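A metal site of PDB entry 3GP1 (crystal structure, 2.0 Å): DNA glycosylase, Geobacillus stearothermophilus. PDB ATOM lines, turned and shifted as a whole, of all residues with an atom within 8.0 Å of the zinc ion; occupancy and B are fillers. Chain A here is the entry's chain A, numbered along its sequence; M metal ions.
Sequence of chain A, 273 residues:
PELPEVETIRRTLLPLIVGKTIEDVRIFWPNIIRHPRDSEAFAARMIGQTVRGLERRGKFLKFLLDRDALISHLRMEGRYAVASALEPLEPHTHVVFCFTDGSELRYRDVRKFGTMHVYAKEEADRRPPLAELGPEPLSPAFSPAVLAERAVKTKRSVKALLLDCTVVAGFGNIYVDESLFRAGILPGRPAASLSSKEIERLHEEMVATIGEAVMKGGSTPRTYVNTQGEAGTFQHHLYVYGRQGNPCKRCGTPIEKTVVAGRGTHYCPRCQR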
ATOM      1  N   PHE A 181      -2.112  13.026  29.381  1.00  0.00           N
ATOM      2  CA  PHE A 181      -2.881  13.326  28.161  1.00  0.00           C
ATOM      3  C   PHE A 181      -4.383  13.420  28.474  1.00  0.00           C
ATOM      4  O   PHE A 181      -5.048  14.405  28.124  1.00  0.00           O
ATOM      5  CB  PHE A 181      -2.656  12.290  27.032  1.00  0.00           C
ATOM      6  CG  PHE A 181      -3.615  12.442  25.889  1.00  0.00           C
ATOM      7  CD1 PHE A 181      -3.400  13.421  24.919  1.00  0.00           C
ATOM      8  CD2 PHE A 181      -4.778  11.681  25.837  1.00  0.00           C
ATOM      9  CE1 PHE A 181      -4.311  13.603  23.878  1.00  0.00           C
ATOM     10  CE2 PHE A 181      -5.689  11.861  24.782  1.00  0.00           C
ATOM     11  CZ  PHE A 181      -5.445  12.830  23.819  1.00  0.00           C
ATOM     12  N   TYR A 239      -3.227   6.667  23.704  1.00  0.00           N
ATOM     13  CA  TYR A 239      -3.408   7.972  23.099  1.00  0.00           C
ATOM     14  C   TYR A 239      -2.090   8.594  22.645  1.00  0.00           C
ATOM     15  O   TYR A 239      -2.022   9.191  21.563  1.00  0.00           O
ATOM     16  CB  TYR A 239      -4.111   8.905  24.080  1.00  0.00           C
ATOM     17  CG  TYR A 239      -5.594   8.598  24.229  1.00  0.00           C
ATOM     18  CD1 TYR A 239      -6.094   8.035  25.406  1.00  0.00           C
ATOM     19  CD2 TYR A 239      -6.486   8.868  23.189  1.00  0.00           C
ATOM     20  CE1 TYR A 239      -7.439   7.740  25.549  1.00  0.00           C
ATOM     21  CE2 TYR A 239      -7.831   8.572  23.318  1.00  0.00           C
ATOM     22  CZ  TYR A 239      -8.302   8.017  24.500  1.00  0.00           C
ATOM     23  OH  TYR A 239      -9.636   7.737  24.619  1.00  0.00           O
ATOM     24  N   VAL A 240      -1.059   8.473  23.487  1.00  0.00           N
ATOM     25  CA  VAL A 240       0.210   9.165  23.218  1.00  0.00           C
ATOM     26  C   VAL A 240       1.462   8.301  23.260  1.00  0.00           C
ATOM     27  O   VAL A 240       2.416   8.575  22.532  1.00  0.00           O
ATOM     28  CB  VAL A 240       0.418  10.443  24.134  1.00  0.00           C
ATOM     29  CG1 VAL A 240      -0.628  11.486  23.866  1.00  0.00           C
ATOM     30  CG2 VAL A 240       0.447  10.095  25.613  1.00  0.00           C
ATOM     31  N   PRO A 247      -0.997  11.254  14.304  1.00  0.00           N
ATOM     32  CA  PRO A 247      -2.042  12.191  14.724  1.00  0.00           C
ATOM     33  C   PRO A 247      -2.638  11.810  16.070  1.00  0.00           C
ATOM     34  O   PRO A 247      -2.827  10.601  16.359  1.00  0.00           O
ATOM     35  CB  PRO A 247      -3.110  12.056  13.619  1.00  0.00           C
ATOM     36  CG  PRO A 247      -2.410  11.444  12.470  1.00  0.00           C
ATOM     37  CD  PRO A 247      -1.374  10.530  13.077  1.00  0.00           C
ATOM     38  N   CYS A 248      -2.885  12.819  16.897  1.00  0.00           N
ATOM     39  CA  CYS A 248      -3.652  12.683  18.107  1.00  0.00           C
ATOM     40  C   CYS A 248      -5.034  12.112  17.762  1.00  0.00           C
ATOM     41  O   CYS A 248      -5.707  12.574  16.823  1.00  0.00           O
ATOM     42  CB  CYS A 248      -3.788  14.030  18.802  1.00  0.00           C
ATOM     43  SG  CYS A 248      -4.792  14.033  20.307  1.00  0.00           S
ATOM     44  N   LYS A 249      -5.432  11.102  18.507  1.00  0.00           N
ATOM     45  CA  LYS A 249      -6.749  10.464  18.363  1.00  0.00           C
ATOM     46  C   LYS A 249      -7.932  11.379  18.683  1.00  0.00           C
ATOM     47  O   LYS A 249      -9.064  11.110  18.258  1.00  0.00           O
ATOM     48  CB  LYS A 249      -6.797   9.173  19.202  1.00  0.00           C
ATOM     49  CG  LYS A 249      -5.866   8.098  18.685  1.00  0.00           C
ATOM     50  CD  LYS A 249      -5.739   6.929  19.651  1.00  0.00           C
ATOM     51  CE  LYS A 249      -4.950   5.784  18.991  1.00  0.00           C
ATOM     52  NZ  LYS A 249      -5.147   4.485  19.671  1.00  0.00           N
ATOM     53  N   ARG A 250      -7.650  12.456  19.433  1.00  0.00           N
ATOM     54  CA  ARG A 250      -8.679  13.402  19.865  1.00  0.00           C
ATOM     55  C   ARG A 250      -8.778  14.662  18.992  1.00  0.00           C
ATOM     56  O   ARG A 250      -9.872  15.154  18.727  1.00  0.00           O
ATOM     57  CB  ARG A 250      -8.446  13.801  21.329  1.00  0.00           C
ATOM     58  CG  ARG A 250      -8.670  12.657  22.331  1.00  0.00           C
ATOM     59  CD  ARG A 250     -10.005  12.811  23.031  1.00  0.00           C
ATOM     60  NE  ARG A 250     -10.339  11.690  23.912  1.00  0.00           N
ATOM     61  CZ  ARG A 250      -9.984  11.602  25.193  1.00  0.00           C
ATOM     62  NH1 ARG A 250      -9.260  12.557  25.760  1.00  0.00           N
ATOM     63  NH2 ARG A 250     -10.352  10.543  25.908  1.00  0.00           N
ATOM     64  N   CYS A 251      -7.634  15.173  18.531  1.00  0.00           N
ATOM     65  CA  CYS A 251      -7.598  16.414  17.757  1.00  0.00           C
ATOM     66  C   CYS A 251      -6.834  16.365  16.431  1.00  0.00           C
ATOM     67  O   CYS A 251      -6.916  17.319  15.666  1.00  0.00           O
ATOM     68  CB  CYS A 251      -7.066  17.581  18.621  1.00  0.00           C
ATOM     69  SG  CYS A 251      -5.289  17.486  18.843  1.00  0.00           S
ATOM     70  N   GLY A 252      -6.105  15.272  16.166  1.00  0.00           N
ATOM     71  CA  GLY A 252      -5.353  15.114  14.906  1.00  0.00           C
ATOM     72  C   GLY A 252      -3.986  15.792  14.822  1.00  0.00           C
ATOM     73  O   GLY A 252      -3.272  15.617  13.823  1.00  0.00           O
ATOM     74  N   THR A 253      -3.612  16.585  15.839  1.00  0.00           N
ATOM     75  CA  THR A 253      -2.271  17.201  15.942  1.00  0.00           C
ATOM     76  C   THR A 253      -1.229  16.108  16.153  1.00  0.00           C
ATOM     77  O   THR A 253      -1.486  15.154  16.907  1.00  0.00           O
ATOM     78  CB  THR A 253      -2.198  18.175  17.164  1.00  0.00           C
ATOM     79  OG1 THR A 253      -3.230  19.158  17.040  1.00  0.00           O
ATOM     80  CG2 THR A 253      -0.814  18.896  17.251  1.00  0.00           C
ATOM     81  N   PRO A 254      -0.067  16.207  15.458  1.00  0.00           N
ATOM     82  CA  PRO A 254       0.906  15.152  15.637  1.00  0.00           C
ATOM     83  C   PRO A 254       1.406  15.068  17.084  1.00  0.00           C
ATOM     84  O   PRO A 254       1.675  16.095  17.735  1.00  0.00           O
ATOM     85  CB  PRO A 254       2.045  15.551  14.678  1.00  0.00           C
ATOM     86  CG  PRO A 254       1.345  16.336  13.600  1.00  0.00           C
ATOM     87  CD  PRO A 254       0.313  17.138  14.367  1.00  0.00           C
ATOM     88  N   ILE A 255       1.522  13.839  17.595  1.00  0.00           N
ATOM     89  CA  ILE A 255       2.005  13.623  18.940  1.00  0.00           C
ATOM     90  C   ILE A 255       3.506  13.935  18.940  1.00  0.00           C
ATOM     91  O   ILE A 255       4.207  13.645  17.966  1.00  0.00           O
ATOM     92  CB  ILE A 255       1.719  12.156  19.391  1.00  0.00           C
ATOM     93  CG1 ILE A 255       0.198  11.919  19.517  1.00  0.00           C
ATOM     94  CG2 ILE A 255       2.474  11.787  20.699  1.00  0.00           C
ATOM     95  CD1 ILE A 255      -0.571  13.033  20.316  1.00  0.00           C
ATOM     96  N   TYR A 267       3.277  13.461  24.341  1.00  0.00           N
ATOM     97  CA  TYR A 267       2.190  14.394  24.627  1.00  0.00           C
ATOM     98  C   TYR A 267       1.631  14.985  23.316  1.00  0.00           C
ATOM     99  O   TYR A 267       2.321  14.996  22.284  1.00  0.00           O
ATOM    100  CB  TYR A 267       2.673  15.527  25.563  1.00  0.00           C
ATOM    101  CG  TYR A 267       3.742  16.396  24.938  1.00  0.00           C
ATOM    102  CD1 TYR A 267       3.396  17.558  24.223  1.00  0.00           C
ATOM    103  CD2 TYR A 267       5.091  16.057  25.058  1.00  0.00           C
ATOM    104  CE1 TYR A 267       4.370  18.334  23.636  1.00  0.00           C
ATOM    105  CE2 TYR A 267       6.080  16.836  24.456  1.00  0.00           C
ATOM    106  CZ  TYR A 267       5.708  17.975  23.752  1.00  0.00           C
ATOM    107  OH  TYR A 267       6.664  18.761  23.165  1.00  0.00           O
ATOM    108  N   CYS A 268       0.378  15.420  23.371  1.00  0.00           N
ATOM    109  CA  CYS A 268      -0.225  16.253  22.341  1.00  0.00           C
ATOM    110  C   CYS A 268      -0.081  17.720  22.731  1.00  0.00           C
ATOM    111  O   CYS A 268      -0.581  18.151  23.793  1.00  0.00           O
ATOM    112  CB  CYS A 268      -1.727  15.902  22.154  1.00  0.00           C
ATOM    113  SG  CYS A 268      -2.511  16.947  20.848  1.00  0.00           S
ATOM    114  N   PRO A 269       0.607  18.524  21.899  1.00  0.00           N
ATOM    115  CA  PRO A 269       0.784  19.929  22.290  1.00  0.00           C
ATOM    116  C   PRO A 269      -0.483  20.805  22.211  1.00  0.00           C
ATOM    117  O   PRO A 269      -0.451  21.960  22.636  1.00  0.00           O
ATOM    118  CB  PRO A 269       1.863  20.421  21.312  1.00  0.00           C
ATOM    119  CG  PRO A 269       1.626  19.599  20.074  1.00  0.00           C
ATOM    120  CD  PRO A 269       1.323  18.213  20.642  1.00  0.00           C
ATOM    121  N   ARG A 270      -1.568  20.277  21.672  1.00  0.00           N
ATOM    122  CA  ARG A 270      -2.837  21.023  21.661  1.00  0.00           C
ATOM    123  C   ARG A 270      -3.742  20.622  22.835  1.00  0.00           C
ATOM    124  O   ARG A 270      -4.311  21.496  23.513  1.00  0.00           O
ATOM    125  CB  ARG A 270      -3.573  20.813  20.343  1.00  0.00           C
ATOM    126  CG  ARG A 270      -4.884  21.578  20.238  1.00  0.00           C
ATOM    127  CD  ARG A 270      -5.550  21.383  18.872  1.00  0.00           C
ATOM    128  NE  ARG A 270      -6.831  22.071  18.871  1.00  0.00           N
ATOM    129  CZ  ARG A 270      -7.622  22.216  17.810  1.00  0.00           C
ATOM    130  NH1 ARG A 270      -8.747  22.905  17.954  1.00  0.00           N
ATOM    131  NH2 ARG A 270      -7.301  21.692  16.625  1.00  0.00           N
ATOM    132  N   CYS A 271      -3.916  19.313  23.030  1.00  0.00           N
ATOM    133  CA  CYS A 271      -4.803  18.796  24.077  1.00  0.00           C
ATOM    134  C   CYS A 271      -4.247  19.063  25.465  1.00  0.00           C
ATOM    135  O   CYS A 271      -5.003  19.224  26.424  1.00  0.00           O
ATOM    136  CB  CYS A 271      -5.058  17.265  23.900  1.00  0.00           C
ATOM    137  SG  CYS A 271      -6.105  16.865  22.440  1.00  0.00           S
ATOM    138  N   GLN A 272      -2.926  19.096  25.589  1.00  0.00           N
ATOM    139  CA  GLN A 272      -2.319  19.268  26.903  1.00  0.00           C
ATOM    140  C   GLN A 272      -1.750  20.656  27.056  1.00  0.00           C
ATOM    141  O   GLN A 272      -1.123  21.163  26.126  1.00  0.00           O
ATOM    142  CB  GLN A 272      -1.238  18.219  27.121  1.00  0.00           C
ATOM    143  CG  GLN A 272      -1.766  16.815  27.127  1.00  0.00           C
ATOM    144  CD  GLN A 272      -0.704  15.748  27.061  1.00  0.00           C
ATOM    145  OE1 GLN A 272      -0.595  15.051  26.065  1.00  0.00           O
ATOM    146  NE2 GLN A 272       0.080  15.595  28.152  1.00  0.00           N
HETATM  147 ZN    ZN M   1      -4.684  16.284  20.763  1.00  0.00          ZN
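N of Arg 270 sits close to SG of Cys 268 (3.6 Å). The backbone NH of Cys 268 lies within hydrogen-bond range of the side-chain amide oxygen of Gln 272 (2.9 Å). The backbone NH (N) of Arg 250 sits close to the side-chain sulfur (SG) of Cys 248. The backbone NH (N) of Cys 248 is in hydrogen-bond range of the backbone carbonyl oxygen (O) of Thr 253 (2.7 Å). SG of Cys 251 lies close to OG1 of Thr 253 (3.2 Å).
The zinc ion is bound by SG of Cys 268. The zinc ion is bound by SG of Cys 271 (2.3 Å). The side-chain sulfur (SG) of Cys 248 binds the zinc ion, at 2.3 Å. SG of Cys 251 is bound to the zinc ion (2.3 Å).
Four residues have an atom within 4 Å of the zinc ion: Cys 248, Cys 251, Cys 268 and Cys 271. The nearest printed residue that does not touch the zinc ion is Phe 181 (4.1 Å).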
